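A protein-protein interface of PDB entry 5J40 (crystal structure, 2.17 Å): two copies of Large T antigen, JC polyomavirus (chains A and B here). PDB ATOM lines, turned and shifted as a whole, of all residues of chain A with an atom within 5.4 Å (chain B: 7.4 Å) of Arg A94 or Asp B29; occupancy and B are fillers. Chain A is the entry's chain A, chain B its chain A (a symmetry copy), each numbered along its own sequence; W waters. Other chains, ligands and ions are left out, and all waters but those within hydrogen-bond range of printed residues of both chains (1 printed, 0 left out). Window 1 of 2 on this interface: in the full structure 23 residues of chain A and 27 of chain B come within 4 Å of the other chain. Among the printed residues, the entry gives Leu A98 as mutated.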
ATOM      1  N   VAL A  89     -24.786   0.148  21.394  1.00  0.00           N
ATOM      2  CA  VAL A  89     -24.570   0.301  22.833  1.00  0.00           C
ATOM      3  C   VAL A  89     -23.109   0.724  23.052  1.00  0.00           C
ATOM      4  O   VAL A  89     -22.871   1.699  23.767  1.00  0.00           O
ATOM      5  CB  VAL A  89     -24.979  -0.962  23.662  1.00  0.00           C
ATOM      6  CG1 VAL A  89     -24.678  -0.775  25.150  1.00  0.00           C
ATOM      7  CG2 VAL A  89     -26.460  -1.293  23.465  1.00  0.00           C
ATOM      8  N   ALA A  90     -22.145   0.038  22.379  1.00  0.00           N
ATOM      9  CA  ALA A  90     -20.714   0.374  22.474  1.00  0.00           C
ATOM     10  C   ALA A  90     -20.435   1.794  21.893  1.00  0.00           C
ATOM     11  O   ALA A  90     -19.602   2.526  22.439  1.00  0.00           O
ATOM     12  CB  ALA A  90     -19.886  -0.671  21.739  1.00  0.00           C
ATOM     13  N   ALA A  91     -21.157   2.177  20.806  1.00  0.00           N
ATOM     14  CA  ALA A  91     -21.086   3.489  20.141  1.00  0.00           C
ATOM     15  C   ALA A  91     -21.525   4.577  21.106  1.00  0.00           C
ATOM     16  O   ALA A  91     -20.880   5.619  21.189  1.00  0.00           O
ATOM     17  CB  ALA A  91     -21.999   3.493  18.915  1.00  0.00           C
ATOM     18  N   LYS A  92     -22.622   4.322  21.850  1.00  0.00           N
ATOM     19  CA  LYS A  92     -23.173   5.214  22.877  1.00  0.00           C
ATOM     20  C   LYS A  92     -22.149   5.391  24.002  1.00  0.00           C
ATOM     21  O   LYS A  92     -21.929   6.513  24.457  1.00  0.00           O
ATOM     22  CB  LYS A  92     -24.480   4.616  23.455  1.00  0.00           C
ATOM     23  CG  LYS A  92     -25.406   5.638  24.079  1.00  0.00           C
ATOM     24  CD  LYS A  92     -25.626   5.365  25.532  1.00  0.00           C
ATOM     25  CE  LYS A  92     -26.554   6.389  26.146  1.00  0.00           C
ATOM     26  NZ  LYS A  92     -26.456   6.380  27.628  1.00  0.00           N
ATOM     27  N   GLN A  93     -21.522   4.293  24.442  1.00  0.00           N
ATOM     28  CA  GLN A  93     -20.465   4.322  25.466  1.00  0.00           C
ATOM     29  C   GLN A  93     -19.272   5.189  25.000  1.00  0.00           C
ATOM     30  O   GLN A  93     -18.714   5.924  25.813  1.00  0.00           O
ATOM     31  CB  GLN A  93     -20.008   2.890  25.832  1.00  0.00           C
ATOM     32  CG  GLN A  93     -20.865   2.119  26.876  1.00  0.00           C
ATOM     33  CD  GLN A  93     -22.251   2.677  27.190  1.00  0.00           C
ATOM     34  OE1 GLN A  93     -22.420   3.584  28.026  1.00  0.00           O
ATOM     35  NE2 GLN A  93     -23.278   2.128  26.544  1.00  0.00           N
ATOM     36  N   ARG A  94     -18.912   5.132  23.692  1.00  0.00           N
ATOM     37  CA  ARG A  94     -17.827   5.947  23.114  1.00  0.00           C
ATOM     38  C   ARG A  94     -18.171   7.430  23.201  1.00  0.00           C
ATOM     39  O   ARG A  94     -17.313   8.253  23.555  1.00  0.00           O
ATOM     40  CB  ARG A  94     -17.570   5.596  21.626  1.00  0.00           C
ATOM     41  CG  ARG A  94     -16.951   4.238  21.409  1.00  0.00           C
ATOM     42  CD  ARG A  94     -15.633   4.393  20.709  1.00  0.00           C
ATOM     43  NE  ARG A  94     -14.616   3.480  21.222  1.00  0.00           N
ATOM     44  CZ  ARG A  94     -13.823   3.752  22.252  1.00  0.00           C
ATOM     45  NH1 ARG A  94     -13.936   4.906  22.900  1.00  0.00           N
ATOM     46  NH2 ARG A  94     -12.921   2.866  22.652  1.00  0.00           N
ATOM     47  N   VAL A  95     -19.419   7.768  22.821  1.00  0.00           N
ATOM     48  CA  VAL A  95     -19.927   9.134  22.854  1.00  0.00           C
ATOM     49  C   VAL A  95     -19.899   9.627  24.301  1.00  0.00           C
ATOM     50  O   VAL A  95     -19.330  10.684  24.559  1.00  0.00           O
ATOM     51  CB  VAL A  95     -21.331   9.256  22.207  1.00  0.00           C
ATOM     52  CG1 VAL A  95     -21.962  10.626  22.488  1.00  0.00           C
ATOM     53  CG2 VAL A  95     -21.252   9.009  20.702  1.00  0.00           C
ATOM     54  N   ASP A  96     -20.459   8.841  25.237  1.00  0.00           N
ATOM     55  CA  ASP A  96     -20.522   9.219  26.655  1.00  0.00           C
ATOM     56  C   ASP A  96     -19.142   9.386  27.286  1.00  0.00           C
ATOM     57  O   ASP A  96     -18.937  10.345  28.011  1.00  0.00           O
ATOM     58  CB  ASP A  96     -21.410   8.250  27.465  1.00  0.00           C
ATOM     59  CG  ASP A  96     -22.872   8.230  27.034  1.00  0.00           C
ATOM     60  OD1 ASP A  96     -23.304   9.171  26.340  1.00  0.00           O
ATOM     61  OD2 ASP A  96     -23.592   7.304  27.430  1.00  0.00           O
ATOM     62  N   SER A  97     -18.174   8.517  26.937  1.00  0.00           N
ATOM     63  CA  SER A  97     -16.812   8.613  27.471  1.00  0.00           C
ATOM     64  C   SER A  97     -16.124   9.905  27.098  1.00  0.00           C
ATOM     65  O   SER A  97     -15.197  10.323  27.785  1.00  0.00           O
ATOM     66  CB  SER A  97     -15.969   7.410  27.066  1.00  0.00           C
ATOM     67  OG  SER A  97     -15.918   7.278  25.655  1.00  0.00           O
ATOM     68  N   LEU A  98     -16.605  10.568  26.053  1.00  0.00           N
ATOM     69  CA  LEU A  98     -16.033  11.832  25.596  1.00  0.00           C
ATOM     70  C   LEU A  98     -16.865  13.056  25.962  1.00  0.00           C
ATOM     71  O   LEU A  98     -16.297  14.129  26.122  1.00  0.00           O
ATOM     72  CB  LEU A  98     -15.786  11.802  24.082  1.00  0.00           C
ATOM     73  CG  LEU A  98     -14.605  10.984  23.537  1.00  0.00           C
ATOM     74  CD1 LEU A  98     -14.648  10.973  22.028  1.00  0.00           C
ATOM     75  CD2 LEU A  98     -13.260  11.581  23.940  1.00  0.00           C
ATOM     76  N   HIS A  99     -18.192  12.913  26.080  1.00  0.00           N
ATOM     77  CA  HIS A  99     -19.091  14.033  26.348  1.00  0.00           C
ATOM     78  C   HIS A  99     -19.656  14.102  27.746  1.00  0.00           C
ATOM     79  O   HIS A  99     -19.907  15.200  28.223  1.00  0.00           O
ATOM     80  CB  HIS A  99     -20.240  14.041  25.329  1.00  0.00           C
ATOM     81  N   ILE A 210     -10.317   0.105  28.823  1.00  0.00           N
ATOM     82  CA  ILE A 210     -10.941   0.941  27.787  1.00  0.00           C
ATOM     83  C   ILE A 210     -12.393   1.328  28.162  1.00  0.00           C
ATOM     84  O   ILE A 210     -13.209   0.462  28.472  1.00  0.00           O
ATOM     85  CB  ILE A 210     -10.801   0.302  26.367  1.00  0.00           C
ATOM     86  CG1 ILE A 210      -9.313   0.320  25.932  1.00  0.00           C
ATOM     87  CG2 ILE A 210     -11.677   1.046  25.325  1.00  0.00           C
ATOM     88  CD1 ILE A 210      -8.906  -0.621  24.811  1.00  0.00           C
ATOM     89  N   ASP A 211     -12.671   2.657  28.182  1.00  0.00           N
ATOM     90  CA  ASP A 211     -13.950   3.303  28.533  1.00  0.00           C
ATOM     91  C   ASP A 211     -14.440   2.985  29.964  1.00  0.00           C
ATOM     92  O   ASP A 211     -15.600   3.242  30.285  1.00  0.00           O
ATOM     93  CB  ASP A 211     -15.058   3.001  27.493  1.00  0.00           C
ATOM     94  CG  ASP A 211     -14.787   3.379  26.042  1.00  0.00           C
ATOM     95  OD1 ASP A 211     -13.988   4.319  25.803  1.00  0.00           O
ATOM     96  OD2 ASP A 211     -15.436   2.792  25.149  1.00  0.00           O
ATOM     97  N   ARG A 262      -7.658   2.197  21.592  1.00  0.00           N
ATOM     98  CA  ARG A 262      -8.090   3.551  21.922  1.00  0.00           C
ATOM     99  C   ARG A 262      -6.970   4.387  22.579  1.00  0.00           C
ATOM    100  O   ARG A 262      -6.163   3.857  23.342  1.00  0.00           O
ATOM    101  CB  ARG A 262      -9.341   3.513  22.838  1.00  0.00           C
ATOM    102  CG  ARG A 262     -10.159   4.814  22.824  1.00  0.00           C
ATOM    103  CD  ARG A 262     -10.838   5.121  24.145  1.00  0.00           C
ATOM    104  NE  ARG A 262     -11.490   6.436  24.123  1.00  0.00           N
ATOM    105  CZ  ARG A 262     -12.106   7.002  25.162  1.00  0.00           C
ATOM    106  NH1 ARG A 262     -12.169   6.374  26.331  1.00  0.00           N
ATOM    107  NH2 ARG A 262     -12.661   8.200  25.039  1.00  0.00           N
ATOM    108  N   ALA B  22     -17.914  12.752   8.840  1.00  0.00           N
ATOM    109  CA  ALA B  22     -16.641  12.179   9.318  1.00  0.00           C
ATOM    110  C   ALA B  22     -15.453  13.045   8.837  1.00  0.00           C
ATOM    111  O   ALA B  22     -14.515  13.248   9.595  1.00  0.00           O
ATOM    112  CB  ALA B  22     -16.483  10.757   8.814  1.00  0.00           C
ATOM    113  N   LYS B  26     -13.028  15.031  11.174  1.00  0.00           N
ATOM    114  CA  LYS B  26     -11.807  14.210  11.132  1.00  0.00           C
ATOM    115  C   LYS B  26     -11.968  12.910  11.966  1.00  0.00           C
ATOM    116  O   LYS B  26     -11.031  12.473  12.649  1.00  0.00           O
ATOM    117  CB  LYS B  26     -10.545  15.020  11.501  1.00  0.00           C
ATOM    118  CG  LYS B  26      -9.371  14.702  10.577  1.00  0.00           C
ATOM    119  CD  LYS B  26      -8.164  14.100  11.305  1.00  0.00           C
ATOM    120  CE  LYS B  26      -7.104  15.135  11.628  1.00  0.00           C
ATOM    121  NZ  LYS B  26      -5.736  14.662  11.275  1.00  0.00           N
ATOM    122  N   CYS B  27     -13.173  12.290  11.879  1.00  0.00           N
ATOM    123  CA  CYS B  27     -13.514  11.079  12.613  1.00  0.00           C
ATOM    124  C   CYS B  27     -12.781   9.828  12.104  1.00  0.00           C
ATOM    125  O   CYS B  27     -12.950   9.413  10.946  1.00  0.00           O
ATOM    126  CB  CYS B  27     -15.027  10.873  12.653  1.00  0.00           C
ATOM    127  SG  CYS B  27     -15.579   9.728  13.938  1.00  0.00           S
ATOM    128  N   GLU B  28     -11.963   9.235  12.993  1.00  0.00           N
ATOM    129  CA  GLU B  28     -11.143   8.037  12.743  1.00  0.00           C
ATOM    130  C   GLU B  28     -11.649   6.790  13.495  1.00  0.00           C
ATOM    131  O   GLU B  28     -11.032   5.720  13.406  1.00  0.00           O
ATOM    132  CB  GLU B  28      -9.688   8.312  13.164  1.00  0.00           C
ATOM    133  CG  GLU B  28      -8.968   9.339  12.311  1.00  0.00           C
ATOM    134  CD  GLU B  28      -7.586   9.723  12.805  1.00  0.00           C
ATOM    135  OE1 GLU B  28      -6.879   8.859  13.378  1.00  0.00           O
ATOM    136  OE2 GLU B  28      -7.201  10.896  12.596  1.00  0.00           O
ATOM    137  N   ASP B  29     -12.764   6.928  14.222  1.00  0.00           N
ATOM    138  CA  ASP B  29     -13.346   5.866  15.043  1.00  0.00           C
ATOM    139  C   ASP B  29     -14.766   5.543  14.550  1.00  0.00           C
ATOM    140  O   ASP B  29     -15.651   6.386  14.613  1.00  0.00           O
ATOM    141  CB  ASP B  29     -13.297   6.317  16.517  1.00  0.00           C
ATOM    142  CG  ASP B  29     -13.848   5.389  17.589  1.00  0.00           C
ATOM    143  OD1 ASP B  29     -14.425   4.329  17.234  1.00  0.00           O
ATOM    144  OD2 ASP B  29     -13.729   5.738  18.783  1.00  0.00           O
ATOM    145  N   VAL B  30     -14.945   4.333  14.005  1.00  0.00           N
ATOM    146  CA  VAL B  30     -16.195   3.789  13.444  1.00  0.00           C
ATOM    147  C   VAL B  30     -17.335   3.853  14.479  1.00  0.00           C
ATOM    148  O   VAL B  30     -18.414   4.323  14.132  1.00  0.00           O
ATOM    149  CB  VAL B  30     -15.989   2.363  12.840  1.00  0.00           C
ATOM    150  CG1 VAL B  30     -17.291   1.767  12.324  1.00  0.00           C
ATOM    151  CG2 VAL B  30     -14.945   2.381  11.728  1.00  0.00           C
ATOM    152  N   PHE B  31     -17.075   3.430  15.745  1.00  0.00           N
ATOM    153  CA  PHE B  31     -18.067   3.449  16.837  1.00  0.00           C
ATOM    154  C   PHE B  31     -18.439   4.856  17.263  1.00  0.00           C
ATOM    155  O   PHE B  31     -19.625   5.132  17.476  1.00  0.00           O
ATOM    156  CB  PHE B  31     -17.618   2.592  18.026  1.00  0.00           C
ATOM    157  CG  PHE B  31     -17.592   1.122  17.673  1.00  0.00           C
ATOM    158  CD1 PHE B  31     -16.483   0.558  17.049  1.00  0.00           C
ATOM    159  CD2 PHE B  31     -18.701   0.316  17.904  1.00  0.00           C
ATOM    160  CE1 PHE B  31     -16.483  -0.779  16.666  1.00  0.00           C
ATOM    161  CE2 PHE B  31     -18.693  -1.029  17.533  1.00  0.00           C
ATOM    162  CZ  PHE B  31     -17.580  -1.572  16.933  1.00  0.00           C
ATOM    163  N   LEU B  32     -17.446   5.773  17.334  1.00  0.00           N
ATOM    164  CA  LEU B  32     -17.714   7.170  17.696  1.00  0.00           C
ATOM    165  C   LEU B  32     -18.580   7.847  16.637  1.00  0.00           C
ATOM    166  O   LEU B  32     -19.532   8.541  16.986  1.00  0.00           O
ATOM    167  CB  LEU B  32     -16.416   7.960  17.934  1.00  0.00           C
ATOM    168  CG  LEU B  32     -16.584   9.399  18.405  1.00  0.00           C
ATOM    169  CD1 LEU B  32     -17.274   9.458  19.783  1.00  0.00           C
ATOM    170  CD2 LEU B  32     -15.260  10.139  18.408  1.00  0.00           C
ATOM    171  N   LEU B  33     -18.303   7.570  15.350  1.00  0.00           N
ATOM    172  CA  LEU B  33     -19.059   8.125  14.228  1.00  0.00           C
ATOM    173  C   LEU B  33     -20.518   7.663  14.299  1.00  0.00           C
ATOM    174  O   LEU B  33     -21.428   8.484  14.181  1.00  0.00           O
ATOM    175  CB  LEU B  33     -18.427   7.703  12.894  1.00  0.00           C
ATOM    176  CG  LEU B  33     -19.161   8.132  11.611  1.00  0.00           C
ATOM    177  CD1 LEU B  33     -19.296   9.626  11.528  1.00  0.00           C
ATOM    178  CD2 LEU B  33     -18.445   7.648  10.401  1.00  0.00           C
ATOM    179  N   MET B  34     -20.718   6.347  14.513  1.00  0.00           N
ATOM    180  CA  MET B  34     -22.011   5.683  14.640  1.00  0.00           C
ATOM    181  C   MET B  34     -22.830   6.361  15.755  1.00  0.00           C
ATOM    182  O   MET B  34     -23.964   6.779  15.527  1.00  0.00           O
ATOM    183  CB  MET B  34     -21.755   4.205  14.954  1.00  0.00           C
ATOM    184  CG  MET B  34     -22.967   3.326  14.857  1.00  0.00           C
ATOM    185  SD  MET B  34     -22.480   1.570  14.703  1.00  0.00           S
ATOM    186  CE  MET B  34     -24.006   0.821  15.103  1.00  0.00           C
ATOM    187  N   GLY B  35     -22.229   6.509  16.927  1.00  0.00           N
ATOM    188  CA  GLY B  35     -22.880   7.136  18.075  1.00  0.00           C
ATOM    189  C   GLY B  35     -23.253   8.587  17.842  1.00  0.00           C
ATOM    190  O   GLY B  35     -24.373   8.989  18.144  1.00  0.00           O
ATOM    191  N   MET B  36     -22.302   9.394  17.335  1.00  0.00           N
ATOM    192  CA  MET B  36     -22.513  10.821  17.000  1.00  0.00           C
ATOM    193  C   MET B  36     -23.616  10.984  15.936  1.00  0.00           C
ATOM    194  O   MET B  36     -24.452  11.876  16.066  1.00  0.00           O
ATOM    195  CB  MET B  36     -21.217  11.460  16.454  1.00  0.00           C
ATOM    196  CG  MET B  36     -20.092  11.593  17.499  1.00  0.00           C
ATOM    197  SD  MET B  36     -20.511  12.523  18.996  1.00  0.00           S
ATOM    198  CE  MET B  36     -20.731  14.168  18.293  1.00  0.00           C
ATOM    199  N   CYS B  82     -20.462   3.519   8.235  1.00  0.00           N
ATOM    200  CA  CYS B  82     -19.460   4.198   9.057  1.00  0.00           C
ATOM    201  C   CYS B  82     -18.033   3.781   8.731  1.00  0.00           C
ATOM    202  O   CYS B  82     -17.140   4.609   8.823  1.00  0.00           O
ATOM    203  CB  CYS B  82     -19.782   4.033  10.544  1.00  0.00           C
ATOM    204  SG  CYS B  82     -21.317   4.855  11.041  1.00  0.00           S
ATOM    205  N   VAL B  86     -15.091   6.337   7.687  1.00  0.00           N
ATOM    206  CA  VAL B  86     -13.804   6.352   8.388  1.00  0.00           C
ATOM    207  C   VAL B  86     -12.633   5.984   7.426  1.00  0.00           C
ATOM    208  O   VAL B  86     -11.545   6.532   7.581  1.00  0.00           O
ATOM    209  CB  VAL B  86     -13.897   5.484   9.670  1.00  0.00           C
ATOM    210  CG1 VAL B  86     -12.523   5.086  10.217  1.00  0.00           C
ATOM    211  CG2 VAL B  86     -14.713   6.220  10.738  1.00  0.00           C
ATOM    212  N   VAL B  89     -11.684   9.152   5.471  1.00  0.00           N
ATOM    213  CA  VAL B  89     -10.907  10.046   6.330  1.00  0.00           C
ATOM    214  C   VAL B  89      -9.441   9.589   6.289  1.00  0.00           C
ATOM    215  O   VAL B  89      -8.562  10.422   6.059  1.00  0.00           O
ATOM    216  CB  VAL B  89     -11.477  10.167   7.783  1.00  0.00           C
ATOM    217  CG1 VAL B  89     -10.596  11.063   8.656  1.00  0.00           C
ATOM    218  CG2 VAL B  89     -12.912  10.697   7.770  1.00  0.00           C
HETATM  219  O   HOH W   1     -14.097   1.960  18.856  1.00  0.00           O
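Position printed for both chains: 89.
Val A89 touches none of the printed residues of chain B.
Of the printed residues of chain B, Ala A91 touches Phe B31 (3.2 Å) and Gly B35 (3.6 Å).
Arg A94 touches just these residues of chain B: Asp B29, Phe B31 and Leu B32.
Printed residues of chain B within 4 Å of Val A95: Gly B35 and Met B36.
Of the printed residues of chain A, Phe B31 touches Ala A91 and Arg A94.
Of the printed residues of chain A, Leu B32 touches Arg A94 and Leu A98.
Met B34 touches none of the printed residues of chain A.
The nearest residue of chain B that does not touch Arg A94 is Val B30 (6.5 Å).
Among the printed residues, merely in contact across the chains: Ala A91 with Phe B31 (3.2 Å), Val A95 with Gly B35 (3.5 Å), Val A95 with Met B36 (3.5 Å), Ala A91 with Gly B35 (3.6 Å), Leu A98 with Leu B32 (3.8 Å), Arg A94 with Phe B31 (3.8 Å) and Arg A94 with Leu B32 (3.96 Å).
Water W1 lies within hydrogen-bond range of the guanidinium group of Arg A94 (2.9 Å) and the side-chain carboxylate of Asp B29 (2.9 Å).
OD2 of Asp B29 lies within salt-bridge range of NE of Arg A94 (3.4 Å).
Of the 15 printed residues of chain B, 5 touch a printed residue of chain A.
Among the printed residues, 8 pairs touch across the chains.
OD1 of Asp B29 sits at hydrogen-bond distance from N of Phe B31.
The side-chain carboxylate (OD1) of Asp A211 is in salt-bridge range of the guanidinium group (NH1) of Arg A94.
The backbone carbonyl oxygen of Arg A94 sits at hydrogen-bond distance from the side-chain hydroxyl of Ser A97, at 2.7 Å.
The backbone NH of Leu B32 lies within hydrogen-bond range of the side-chain carboxylate of Asp B29, at 3.3 Å.
The side-chain sulfur of Cys B27 lies within hydrogen-bond range of the backbone carbonyl oxygen of Asp B29.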
